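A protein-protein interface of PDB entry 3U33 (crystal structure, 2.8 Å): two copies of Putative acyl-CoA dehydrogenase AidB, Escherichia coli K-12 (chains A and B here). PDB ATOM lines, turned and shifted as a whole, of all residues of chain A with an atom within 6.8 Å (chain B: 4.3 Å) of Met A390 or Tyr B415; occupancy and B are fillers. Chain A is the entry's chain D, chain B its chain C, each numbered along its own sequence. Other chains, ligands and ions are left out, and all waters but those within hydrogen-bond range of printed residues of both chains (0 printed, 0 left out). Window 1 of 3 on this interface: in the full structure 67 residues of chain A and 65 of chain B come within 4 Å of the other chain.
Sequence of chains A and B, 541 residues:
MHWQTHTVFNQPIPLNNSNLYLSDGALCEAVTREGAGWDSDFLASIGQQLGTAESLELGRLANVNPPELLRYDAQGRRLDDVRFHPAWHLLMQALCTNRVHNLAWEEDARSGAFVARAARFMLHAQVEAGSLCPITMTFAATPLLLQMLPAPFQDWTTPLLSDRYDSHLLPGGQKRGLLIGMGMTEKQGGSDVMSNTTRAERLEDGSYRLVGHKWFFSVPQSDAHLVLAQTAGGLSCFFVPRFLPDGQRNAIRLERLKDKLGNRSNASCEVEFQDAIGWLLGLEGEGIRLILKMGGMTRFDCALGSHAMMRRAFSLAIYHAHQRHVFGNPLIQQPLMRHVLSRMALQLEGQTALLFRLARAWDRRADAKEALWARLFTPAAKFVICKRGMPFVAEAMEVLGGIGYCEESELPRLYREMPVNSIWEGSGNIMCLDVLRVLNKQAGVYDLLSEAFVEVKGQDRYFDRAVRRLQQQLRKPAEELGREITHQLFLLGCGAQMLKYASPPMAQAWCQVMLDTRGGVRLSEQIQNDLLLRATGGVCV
The backbone carbonyl oxygen (O) of Arg B416 sits at hydrogen-bond distance from the side-chain hydroxyl (OH) of Tyr A405 (2.9 Å).
OH of Tyr A415 is in hydrogen-bond range of O of Tyr B415, 2.6 Å away.
The backbone carbonyl oxygen (O) of Leu A261 lies within hydrogen-bond range of the guanidinium group (NH1) of Arg A416 (3.0 Å).
Among the printed residues, pairs that only touch across the chains: Met A390 with Tyr B415 (3.4 Å), Leu A261 with Tyr B415 (3.4 Å), Tyr A415 with Pro B419 (3.5 Å), Pro A419 with Tyr B415 (3.6 Å), Leu A261 with Arg B416 (3.6 Å), Leu A261 with Met B397 (3.7 Å), Tyr A405 with Glu B417 (3.8 Å), Arg A416 with Arg B416 (3.9 Å), Met A390 with Ala B394 (3.9 Å) and Pro A419 with Met B397 (3.99 Å).
Of the printed residues of chain B, Leu A261 touches Met B397, Tyr B415 and Arg B416.
Of the printed residues of chain B, Tyr A405 touches Arg B416 and Glu B417.
Of the printed residues of chain B, Pro A419 touches Met B397 and Tyr B415.
Val B393 touches none of the printed residues of chain A.
Pro B412 touches none of the printed residues of chain A.
Of chain A, only Leu A261 (3.4 Å), Met A390 (3.4 Å), Tyr A415 (2.6 Å) and Pro A419 (3.6 Å) come within 4 Å of Tyr B415.
Printed residues of chain A within 4 Å of Arg B416: Leu A261, Tyr A405 and Arg A416.
The nearest residue of chain A that does not touch Tyr B415 is Arg A416 (4.3 Å).
The nearest printed residue of chain B that does not touch Leu A261 is Pro B412 (4.1 Å).
Along chain B the printed residues that touch a printed residue of chain A span positions 394 to 419.
Among the printed residues, 12 pairs touch across the chains.
Tyr B415 touches its own counterpart, Tyr A415.
Tyr A415 touches Pro B419, and with the chains exchanged Pro A419 touches Tyr B415.
Arg A416 touches its own counterpart, Arg B416.
Positions printed for both chains: 393, 394, 412, 414, 415, 416, 417, 418 and 419.
Of the 12 pairs that touch across the chains among the printed residues, 4 have their exchanged pair printed and touching as well.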
ATOM      1  N   LEU A 261      36.748 -11.651   0.091  1.00  0.00           N
ATOM      2  CA  LEU A 261      36.116 -10.933   1.193  1.00  0.00           C
ATOM      3  C   LEU A 261      36.047 -11.824   2.426  1.00  0.00           C
ATOM      4  O   LEU A 261      36.509 -11.459   3.504  1.00  0.00           O
ATOM      5  CB  LEU A 261      34.707 -10.497   0.787  1.00  0.00           C
ATOM      6  CG  LEU A 261      33.766 -10.035   1.902  1.00  0.00           C
ATOM      7  CD1 LEU A 261      34.439  -9.024   2.811  1.00  0.00           C
ATOM      8  CD2 LEU A 261      32.489  -9.455   1.314  1.00  0.00           C
ATOM      9  N   SER A 306      24.344 -21.096   5.524  1.00  0.00           N
ATOM     10  CA  SER A 306      23.928 -19.753   5.891  1.00  0.00           C
ATOM     11  C   SER A 306      23.113 -19.795   7.180  1.00  0.00           C
ATOM     12  O   SER A 306      23.326 -18.995   8.089  1.00  0.00           O
ATOM     13  CB  SER A 306      23.125 -19.101   4.764  1.00  0.00           C
ATOM     14  OG  SER A 306      23.979 -18.539   3.785  1.00  0.00           O
ATOM     15  N   MET A 310      23.922 -18.027  10.802  1.00  0.00           N
ATOM     16  CA  MET A 310      22.954 -17.155  11.451  1.00  0.00           C
ATOM     17  C   MET A 310      22.702 -17.650  12.869  1.00  0.00           C
ATOM     18  O   MET A 310      22.601 -16.854  13.803  1.00  0.00           O
ATOM     19  CB  MET A 310      21.656 -17.099  10.656  1.00  0.00           C
ATOM     20  CG  MET A 310      21.835 -16.556   9.248  1.00  0.00           C
ATOM     21  SD  MET A 310      20.421 -16.824   8.156  1.00  0.00           S
ATOM     22  CE  MET A 310      19.222 -15.717   8.870  1.00  0.00           C
ATOM     23  N   ILE A 385      17.003 -17.881   2.428  1.00  0.00           N
ATOM     24  CA  ILE A 385      17.849 -17.990   3.613  1.00  0.00           C
ATOM     25  C   ILE A 385      19.196 -17.286   3.394  1.00  0.00           C
ATOM     26  O   ILE A 385      19.626 -16.471   4.210  1.00  0.00           O
ATOM     27  CB  ILE A 385      18.057 -19.457   4.051  1.00  0.00           C
ATOM     28  CG1 ILE A 385      16.722 -20.081   4.449  1.00  0.00           C
ATOM     29  CG2 ILE A 385      19.002 -19.528   5.219  1.00  0.00           C
ATOM     30  CD1 ILE A 385      16.831 -21.501   4.983  1.00  0.00           C
ATOM     31  N   CYS A 386      19.851 -17.589   2.282  1.00  0.00           N
ATOM     32  CA  CYS A 386      21.138 -16.979   2.000  1.00  0.00           C
ATOM     33  C   CYS A 386      21.059 -15.456   1.879  1.00  0.00           C
ATOM     34  O   CYS A 386      22.021 -14.760   2.187  1.00  0.00           O
ATOM     35  CB  CYS A 386      21.763 -17.599   0.753  1.00  0.00           C
ATOM     36  SG  CYS A 386      22.290 -19.304   1.006  1.00  0.00           S
ATOM     37  N   LYS A 387      19.916 -14.942   1.437  1.00  0.00           N
ATOM     38  CA  LYS A 387      19.701 -13.500   1.356  1.00  0.00           C
ATOM     39  C   LYS A 387      19.510 -12.885   2.759  1.00  0.00           C
ATOM     40  O   LYS A 387      20.038 -11.806   3.058  1.00  0.00           O
ATOM     41  CB  LYS A 387      18.482 -13.205   0.482  1.00  0.00           C
ATOM     42  CG  LYS A 387      18.661 -12.065  -0.499  1.00  0.00           C
ATOM     43  CD  LYS A 387      19.520 -12.509  -1.668  1.00  0.00           C
ATOM     44  CE  LYS A 387      19.728 -11.391  -2.679  1.00  0.00           C
ATOM     45  NZ  LYS A 387      20.503 -11.853  -3.864  1.00  0.00           N
ATOM     46  N   ARG A 388      18.749 -13.577   3.606  1.00  0.00           N
ATOM     47  CA  ARG A 388      18.531 -13.161   4.987  1.00  0.00           C
ATOM     48  C   ARG A 388      19.827 -13.140   5.785  1.00  0.00           C
ATOM     49  O   ARG A 388      19.936 -12.423   6.782  1.00  0.00           O
ATOM     50  CB  ARG A 388      17.566 -14.108   5.690  1.00  0.00           C
ATOM     51  CG  ARG A 388      16.098 -13.871   5.419  1.00  0.00           C
ATOM     52  CD  ARG A 388      15.285 -14.932   6.141  1.00  0.00           C
ATOM     53  NE  ARG A 388      13.848 -14.819   5.919  1.00  0.00           N
ATOM     54  CZ  ARG A 388      12.964 -15.685   6.400  1.00  0.00           C
ATOM     55  NH1 ARG A 388      13.382 -16.723   7.114  1.00  0.00           N
ATOM     56  NH2 ARG A 388      11.667 -15.522   6.166  1.00  0.00           N
ATOM     57  N   GLY A 389      20.802 -13.937   5.356  1.00  0.00           N
ATOM     58  CA  GLY A 389      22.052 -14.070   6.084  1.00  0.00           C
ATOM     59  C   GLY A 389      22.708 -12.749   6.450  1.00  0.00           C
ATOM     60  O   GLY A 389      23.054 -12.503   7.609  1.00  0.00           O
ATOM     61  N   MET A 390      22.873 -11.896   5.447  1.00  0.00           N
ATOM     62  CA  MET A 390      23.555 -10.619   5.622  1.00  0.00           C
ATOM     63  C   MET A 390      22.918  -9.694   6.672  1.00  0.00           C
ATOM     64  O   MET A 390      23.576  -9.312   7.630  1.00  0.00           O
ATOM     65  CB  MET A 390      23.712  -9.905   4.270  1.00  0.00           C
ATOM     66  CG  MET A 390      24.800 -10.484   3.369  1.00  0.00           C
ATOM     67  SD  MET A 390      24.408 -12.093   2.650  1.00  0.00           S
ATOM     68  CE  MET A 390      23.266 -11.640   1.353  1.00  0.00           C
ATOM     69  N   PRO A 391      21.641  -9.323   6.493  1.00  0.00           N
ATOM     70  CA  PRO A 391      21.009  -8.424   7.466  1.00  0.00           C
ATOM     71  C   PRO A 391      20.979  -9.028   8.867  1.00  0.00           C
ATOM     72  O   PRO A 391      21.161  -8.318   9.856  1.00  0.00           O
ATOM     73  CB  PRO A 391      19.572  -8.292   6.944  1.00  0.00           C
ATOM     74  CG  PRO A 391      19.628  -8.686   5.512  1.00  0.00           C
ATOM     75  CD  PRO A 391      20.717  -9.707   5.410  1.00  0.00           C
ATOM     76  N   PHE A 392      20.745 -10.334   8.935  1.00  0.00           N
ATOM     77  CA  PHE A 392      20.617 -11.051  10.196  1.00  0.00           C
ATOM     78  C   PHE A 392      21.914 -10.983  10.997  1.00  0.00           C
ATOM     79  O   PHE A 392      21.918 -10.559  12.152  1.00  0.00           O
ATOM     80  CB  PHE A 392      20.233 -12.514   9.922  1.00  0.00           C
ATOM     81  CG  PHE A 392      19.803 -13.286  11.147  1.00  0.00           C
ATOM     82  CD1 PHE A 392      20.744 -13.854  11.995  1.00  0.00           C
ATOM     83  CD2 PHE A 392      18.456 -13.472  11.425  1.00  0.00           C
ATOM     84  CE1 PHE A 392      20.351 -14.566  13.101  1.00  0.00           C
ATOM     85  CE2 PHE A 392      18.054 -14.180  12.530  1.00  0.00           C
ATOM     86  CZ  PHE A 392      19.001 -14.729  13.374  1.00  0.00           C
ATOM     87  N   VAL A 393      23.014 -11.401  10.379  1.00  0.00           N
ATOM     88  CA  VAL A 393      24.297 -11.425  11.071  1.00  0.00           C
ATOM     89  C   VAL A 393      24.734 -10.011  11.426  1.00  0.00           C
ATOM     90  O   VAL A 393      25.334  -9.781  12.476  1.00  0.00           O
ATOM     91  CB  VAL A 393      25.386 -12.114  10.238  1.00  0.00           C
ATOM     92  CG1 VAL A 393      26.729 -11.990  10.927  1.00  0.00           C
ATOM     93  CG2 VAL A 393      25.037 -13.570  10.022  1.00  0.00           C
ATOM     94  N   ALA A 394      24.425  -9.064  10.550  1.00  0.00           N
ATOM     95  CA  ALA A 394      24.704  -7.664  10.821  1.00  0.00           C
ATOM     96  C   ALA A 394      23.982  -7.207  12.084  1.00  0.00           C
ATOM     97  O   ALA A 394      24.522  -6.425  12.863  1.00  0.00           O
ATOM     98  CB  ALA A 394      24.304  -6.801   9.639  1.00  0.00           C
ATOM     99  N   GLU A 395      22.759  -7.699  12.278  1.00  0.00           N
ATOM    100  CA  GLU A 395      21.988  -7.370  13.474  1.00  0.00           C
ATOM    101  C   GLU A 395      22.661  -7.950  14.707  1.00  0.00           C
ATOM    102  O   GLU A 395      22.858  -7.254  15.704  1.00  0.00           O
ATOM    103  CB  GLU A 395      20.562  -7.899  13.370  1.00  0.00           C
ATOM    104  CG  GLU A 395      19.646  -7.353  14.435  1.00  0.00           C
ATOM    105  CD  GLU A 395      19.381  -5.866  14.268  1.00  0.00           C
ATOM    106  OE1 GLU A 395      18.838  -5.473  13.210  1.00  0.00           O
ATOM    107  OE2 GLU A 395      19.714  -5.090  15.195  1.00  0.00           O
ATOM    108  N   TYR A 405      32.376  -5.308  15.824  1.00  0.00           N
ATOM    109  CA  TYR A 405      32.878  -4.815  14.551  1.00  0.00           C
ATOM    110  C   TYR A 405      34.376  -5.036  14.468  1.00  0.00           C
ATOM    111  O   TYR A 405      35.005  -4.661  13.475  1.00  0.00           O
ATOM    112  CB  TYR A 405      32.545  -3.331  14.396  1.00  0.00           C
ATOM    113  CG  TYR A 405      32.833  -2.761  13.027  1.00  0.00           C
ATOM    114  CD1 TYR A 405      33.876  -1.859  12.831  1.00  0.00           C
ATOM    115  CD2 TYR A 405      32.059  -3.113  11.931  1.00  0.00           C
ATOM    116  CE1 TYR A 405      34.138  -1.329  11.585  1.00  0.00           C
ATOM    117  CE2 TYR A 405      32.314  -2.586  10.679  1.00  0.00           C
ATOM    118  CZ  TYR A 405      33.358  -1.697  10.510  1.00  0.00           C
ATOM    119  OH  TYR A 405      33.615  -1.172   9.265  1.00  0.00           O
ATOM    120  N   PRO A 412      32.611 -10.455  12.569  1.00  0.00           N
ATOM    121  CA  PRO A 412      33.077  -9.993  11.254  1.00  0.00           C
ATOM    122  C   PRO A 412      33.342 -11.136  10.272  1.00  0.00           C
ATOM    123  O   PRO A 412      32.935 -11.048   9.120  1.00  0.00           O
ATOM    124  CB  PRO A 412      34.374  -9.254  11.586  1.00  0.00           C
ATOM    125  CG  PRO A 412      34.163  -8.774  12.980  1.00  0.00           C
ATOM    126  CD  PRO A 412      33.388  -9.863  13.668  1.00  0.00           C
ATOM    127  N   LEU A 414      31.975 -14.075  10.165  1.00  0.00           N
ATOM    128  CA  LEU A 414      30.664 -14.567   9.759  1.00  0.00           C
ATOM    129  C   LEU A 414      30.027 -13.605   8.766  1.00  0.00           C
ATOM    130  O   LEU A 414      29.594 -14.001   7.687  1.00  0.00           O
ATOM    131  CB  LEU A 414      29.744 -14.728  10.975  1.00  0.00           C
ATOM    132  CG  LEU A 414      30.046 -15.852  11.969  1.00  0.00           C
ATOM    133  CD1 LEU A 414      29.286 -15.620  13.261  1.00  0.00           C
ATOM    134  CD2 LEU A 414      29.699 -17.214  11.384  1.00  0.00           C
ATOM    135  N   TYR A 415      29.971 -12.335   9.148  1.00  0.00           N
ATOM    136  CA  TYR A 415      29.417 -11.294   8.300  1.00  0.00           C
ATOM    137  C   TYR A 415      30.080 -11.289   6.926  1.00  0.00           C
ATOM    138  O   TYR A 415      29.423 -11.038   5.915  1.00  0.00           O
ATOM    139  CB  TYR A 415      29.581  -9.925   8.970  1.00  0.00           C
ATOM    140  CG  TYR A 415      29.162  -8.755   8.106  1.00  0.00           C
ATOM    141  CD1 TYR A 415      27.819  -8.447   7.919  1.00  0.00           C
ATOM    142  CD2 TYR A 415      30.105  -7.955   7.485  1.00  0.00           C
ATOM    143  CE1 TYR A 415      27.431  -7.379   7.131  1.00  0.00           C
ATOM    144  CE2 TYR A 415      29.725  -6.887   6.695  1.00  0.00           C
ATOM    145  CZ  TYR A 415      28.391  -6.606   6.522  1.00  0.00           C
ATOM    146  OH  TYR A 415      28.015  -5.543   5.738  1.00  0.00           O
ATOM    147  N   ARG A 416      31.382 -11.565   6.900  1.00  0.00           N
ATOM    148  CA  ARG A 416      32.144 -11.560   5.657  1.00  0.00           C
ATOM    149  C   ARG A 416      31.900 -12.828   4.841  1.00  0.00           C
ATOM    150  O   ARG A 416      32.199 -12.874   3.643  1.00  0.00           O
ATOM    151  CB  ARG A 416      33.640 -11.378   5.929  1.00  0.00           C
ATOM    152  CG  ARG A 416      34.037  -9.963   6.310  1.00  0.00           C
ATOM    153  CD  ARG A 416      35.563  -9.790   6.366  1.00  0.00           C
ATOM    154  NE  ARG A 416      36.199 -10.465   7.502  1.00  0.00           N
ATOM    155  CZ  ARG A 416      36.702 -11.696   7.453  1.00  0.00           C
ATOM    156  NH1 ARG A 416      36.642 -12.391   6.327  1.00  0.00           N
ATOM    157  NH2 ARG A 416      37.257 -12.242   8.530  1.00  0.00           N
ATOM    158  N   GLU A 417      31.346 -13.847   5.490  1.00  0.00           N
ATOM    159  CA  GLU A 417      31.121 -15.134   4.837  1.00  0.00           C
ATOM    160  C   GLU A 417      29.787 -15.158   4.105  1.00  0.00           C
ATOM    161  O   GLU A 417      29.672 -15.708   3.006  1.00  0.00           O
ATOM    162  CB  GLU A 417      31.145 -16.263   5.865  1.00  0.00           C
ATOM    163  CG  GLU A 417      31.171 -17.647   5.267  1.00  0.00           C
ATOM    164  CD  GLU A 417      32.525 -18.008   4.692  1.00  0.00           C
ATOM    165  OE1 GLU A 417      33.527 -17.371   5.094  1.00  0.00           O
ATOM    166  OE2 GLU A 417      32.586 -18.929   3.845  1.00  0.00           O
ATOM    167  N   MET A 418      28.789 -14.533   4.718  1.00  0.00           N
ATOM    168  CA  MET A 418      27.404 -14.660   4.280  1.00  0.00           C
ATOM    169  C   MET A 418      27.165 -14.525   2.775  1.00  0.00           C
ATOM    170  O   MET A 418      26.440 -15.329   2.200  1.00  0.00           O
ATOM    171  CB  MET A 418      26.503 -13.701   5.062  1.00  0.00           C
ATOM    172  CG  MET A 418      26.636 -13.819   6.584  1.00  0.00           C
ATOM    173  SD  MET A 418      26.485 -15.500   7.233  1.00  0.00           S
ATOM    174  CE  MET A 418      24.793 -15.879   6.799  1.00  0.00           C
ATOM    175  N   PRO A 419      27.767 -13.516   2.131  1.00  0.00           N
ATOM    176  CA  PRO A 419      27.443 -13.289   0.717  1.00  0.00           C
ATOM    177  C   PRO A 419      27.888 -14.420  -0.204  1.00  0.00           C
ATOM    178  O   PRO A 419      27.292 -14.620  -1.264  1.00  0.00           O
ATOM    179  CB  PRO A 419      28.223 -12.012   0.379  1.00  0.00           C
ATOM    180  CG  PRO A 419      28.447 -11.349   1.688  1.00  0.00           C
ATOM    181  CD  PRO A 419      28.652 -12.468   2.658  1.00  0.00           C
ATOM    182  N   VAL A 420      28.929 -15.145   0.185  1.00  0.00           N
ATOM    183  CA  VAL A 420      29.444 -16.196  -0.681  1.00  0.00           C
ATOM    184  C   VAL A 420      28.383 -17.265  -0.934  1.00  0.00           C
ATOM    185  O   VAL A 420      28.227 -17.736  -2.055  1.00  0.00           O
ATOM    186  CB  VAL A 420      30.744 -16.817  -0.135  1.00  0.00           C
ATOM    187  CG1 VAL A 420      30.439 -17.870   0.899  1.00  0.00           C
ATOM    188  CG2 VAL A 420      31.565 -17.408  -1.276  1.00  0.00           C
ATOM    189  N   SER A 422      25.223 -16.871  -1.016  1.00  0.00           N
ATOM    190  CA  SER A 422      24.185 -16.327  -1.880  1.00  0.00           C
ATOM    191  C   SER A 422      24.638 -16.223  -3.336  1.00  0.00           C
ATOM    192  O   SER A 422      23.812 -16.205  -4.243  1.00  0.00           O
ATOM    193  CB  SER A 422      23.734 -14.960  -1.371  1.00  0.00           C
ATOM    194  OG  SER A 422      22.637 -14.484  -2.124  1.00  0.00           O
ATOM    195  N   VAL B 393      24.059  -3.152  -0.398  1.00  0.00           N
ATOM    196  CA  VAL B 393      25.384  -3.303  -0.967  1.00  0.00           C
ATOM    197  C   VAL B 393      25.643  -4.761  -1.314  1.00  0.00           C
ATOM    198  O   VAL B 393      26.237  -5.067  -2.350  1.00  0.00           O
ATOM    199  CB  VAL B 393      26.471  -2.778  -0.022  1.00  0.00           C
ATOM    200  CG1 VAL B 393      27.843  -3.128  -0.560  1.00  0.00           C
ATOM    201  CG2 VAL B 393      26.327  -1.274   0.130  1.00  0.00           C
ATOM    202  N   ALA B 394      25.187  -5.658  -0.446  1.00  0.00           N
ATOM    203  CA  ALA B 394      25.303  -7.089  -0.699  1.00  0.00           C
ATOM    204  C   ALA B 394      24.689  -7.432  -2.054  1.00  0.00           C
ATOM    205  O   ALA B 394      25.283  -8.166  -2.844  1.00  0.00           O
ATOM    206  CB  ALA B 394      24.631  -7.885   0.416  1.00  0.00           C
ATOM    207  N   MET B 397      26.799  -6.264  -4.885  1.00  0.00           N
ATOM    208  CA  MET B 397      27.910  -7.194  -4.994  1.00  0.00           C
ATOM    209  C   MET B 397      27.522  -8.420  -5.800  1.00  0.00           C
ATOM    210  O   MET B 397      28.298  -8.906  -6.623  1.00  0.00           O
ATOM    211  CB  MET B 397      28.364  -7.621  -3.599  1.00  0.00           C
ATOM    212  CG  MET B 397      29.487  -8.629  -3.582  1.00  0.00           C
ATOM    213  SD  MET B 397      29.843  -9.165  -1.901  1.00  0.00           S
ATOM    214  CE  MET B 397      30.422  -7.627  -1.175  1.00  0.00           C
ATOM    215  N   LEU B 411      33.581  -3.425  -4.011  1.00  0.00           N
ATOM    216  CA  LEU B 411      32.395  -3.898  -3.291  1.00  0.00           C
ATOM    217  C   LEU B 411      32.649  -4.431  -1.873  1.00  0.00           C
ATOM    218  O   LEU B 411      31.962  -4.028  -0.932  1.00  0.00           O
ATOM    219  CB  LEU B 411      31.595  -4.908  -4.125  1.00  0.00           C
ATOM    220  CG  LEU B 411      30.586  -4.305  -5.106  1.00  0.00           C
ATOM    221  CD1 LEU B 411      29.598  -3.405  -4.383  1.00  0.00           C
ATOM    222  CD2 LEU B 411      31.293  -3.530  -6.197  1.00  0.00           C
ATOM    223  N   PRO B 412      33.616  -5.346  -1.711  1.00  0.00           N
ATOM    224  CA  PRO B 412      33.919  -5.838  -0.363  1.00  0.00           C
ATOM    225  C   PRO B 412      34.195  -4.704   0.628  1.00  0.00           C
ATOM    226  O   PRO B 412      33.683  -4.734   1.745  1.00  0.00           O
ATOM    227  CB  PRO B 412      35.180  -6.677  -0.575  1.00  0.00           C
ATOM    228  CG  PRO B 412      35.042  -7.175  -1.969  1.00  0.00           C
ATOM    229  CD  PRO B 412      34.378  -6.064  -2.746  1.00  0.00           C
ATOM    230  N   ARG B 413      34.992  -3.716   0.229  1.00  0.00           N
ATOM    231  CA  ARG B 413      35.314  -2.610   1.118  1.00  0.00           C
ATOM    232  C   ARG B 413      34.060  -1.837   1.499  1.00  0.00           C
ATOM    233  O   ARG B 413      33.894  -1.442   2.651  1.00  0.00           O
ATOM    234  CB  ARG B 413      36.358  -1.689   0.483  1.00  0.00           C
ATOM    235  CG  ARG B 413      36.742  -0.479   1.341  1.00  0.00           C
ATOM    236  CD  ARG B 413      38.083   0.088   0.905  1.00  0.00           C
ATOM    237  NE  ARG B 413      38.131   0.373  -0.529  1.00  0.00           N
ATOM    238  CZ  ARG B 413      37.794   1.541  -1.067  1.00  0.00           C
ATOM    239  NH1 ARG B 413      37.381   2.535  -0.290  1.00  0.00           N
ATOM    240  NH2 ARG B 413      37.872   1.720  -2.378  1.00  0.00           N
ATOM    241  N   LEU B 414      33.178  -1.629   0.531  1.00  0.00           N
ATOM    242  CA  LEU B 414      31.895  -0.986   0.796  1.00  0.00           C
ATOM    243  C   LEU B 414      31.055  -1.837   1.744  1.00  0.00           C
ATOM    244  O   LEU B 414      30.561  -1.350   2.762  1.00  0.00           O
ATOM    245  CB  LEU B 414      31.132  -0.737  -0.512  1.00  0.00           C
ATOM    246  CG  LEU B 414      31.626   0.413  -1.394  1.00  0.00           C
ATOM    247  CD1 LEU B 414      31.018   0.317  -2.788  1.00  0.00           C
ATOM    248  CD2 LEU B 414      31.330   1.768  -0.753  1.00  0.00           C
ATOM    249  N   TYR B 415      30.907  -3.112   1.394  1.00  0.00           N
ATOM    250  CA  TYR B 415      30.151  -4.066   2.196  1.00  0.00           C
ATOM    251  C   TYR B 415      30.693  -4.150   3.618  1.00  0.00           C
ATOM    252  O   TYR B 415      29.930  -4.329   4.566  1.00  0.00           O
ATOM    253  CB  TYR B 415      30.184  -5.445   1.543  1.00  0.00           C
ATOM    254  CG  TYR B 415      29.551  -6.530   2.374  1.00  0.00           C
ATOM    255  CD1 TYR B 415      28.169  -6.652   2.451  1.00  0.00           C
ATOM    256  CD2 TYR B 415      30.330  -7.439   3.076  1.00  0.00           C
ATOM    257  CE1 TYR B 415      27.577  -7.645   3.208  1.00  0.00           C
ATOM    258  CE2 TYR B 415      29.746  -8.437   3.836  1.00  0.00           C
ATOM    259  CZ  TYR B 415      28.369  -8.535   3.901  1.00  0.00           C
ATOM    260  OH  TYR B 415      27.784  -9.525   4.661  1.00  0.00           O
ATOM    261  N   ARG B 416      32.009  -4.010   3.755  1.00  0.00           N
ATOM    262  CA  ARG B 416      32.655  -4.070   5.060  1.00  0.00           C
ATOM    263  C   ARG B 416      32.475  -2.790   5.872  1.00  0.00           C
ATOM    264  O   ARG B 416      32.521  -2.818   7.097  1.00  0.00           O
ATOM    265  CB  ARG B 416      34.138  -4.414   4.913  1.00  0.00           C
ATOM    266  CG  ARG B 416      34.399  -5.877   4.597  1.00  0.00           C
ATOM    267  CD  ARG B 416      35.862  -6.251   4.757  1.00  0.00           C
ATOM    268  NE  ARG B 416      36.683  -5.780   3.644  1.00  0.00           N
ATOM    269  CZ  ARG B 416      37.426  -4.678   3.671  1.00  0.00           C
ATOM    270  NH1 ARG B 416      37.457  -3.917   4.758  1.00  0.00           N
ATOM    271  NH2 ARG B 416      38.136  -4.333   2.608  1.00  0.00           N
ATOM    272  N   GLU B 417      32.264  -1.674   5.184  1.00  0.00           N
ATOM    273  CA  GLU B 417      32.121  -0.383   5.843  1.00  0.00           C
ATOM    274  C   GLU B 417      30.728  -0.215   6.432  1.00  0.00           C
ATOM    275  O   GLU B 417      30.566   0.330   7.526  1.00  0.00           O
ATOM    276  CB  GLU B 417      32.385   0.741   4.843  1.00  0.00           C
ATOM    277  CG  GLU B 417      32.476   2.137   5.457  1.00  0.00           C
ATOM    278  CD  GLU B 417      33.806   2.401   6.161  1.00  0.00           C
ATOM    279  OE1 GLU B 417      34.839   1.807   5.759  1.00  0.00           O
ATOM    280  OE2 GLU B 417      33.810   3.208   7.119  1.00  0.00           O
ATOM    281  N   MET B 418      29.727  -0.702   5.703  1.00  0.00           N
ATOM    282  CA  MET B 418      28.326  -0.431   6.011  1.00  0.00           C
ATOM    283  C   MET B 418      27.893  -0.509   7.479  1.00  0.00           C
ATOM    284  O   MET B 418      27.223   0.397   7.962  1.00  0.00           O
ATOM    285  CB  MET B 418      27.414  -1.304   5.148  1.00  0.00           C
ATOM    286  CG  MET B 418      27.722  -1.249   3.650  1.00  0.00           C
ATOM    287  SD  MET B 418      27.759   0.407   2.959  1.00  0.00           S
ATOM    288  CE  MET B 418      26.094   0.968   3.280  1.00  0.00           C
ATOM    289  N   PRO B 419      28.252  -1.593   8.189  1.00  0.00           N
ATOM    290  CA  PRO B 419      27.734  -1.755   9.558  1.00  0.00           C
ATOM    291  C   PRO B 419      28.248  -0.688  10.526  1.00  0.00           C
ATOM    292  O   PRO B 419      27.593  -0.393  11.536  1.00  0.00           O
ATOM    293  CB  PRO B 419      28.260  -3.135   9.987  1.00  0.00           C
ATOM    294  CG  PRO B 419      28.651  -3.814   8.735  1.00  0.00           C
ATOM    295  CD  PRO B 419      29.093  -2.733   7.789  1.00  0.00           C
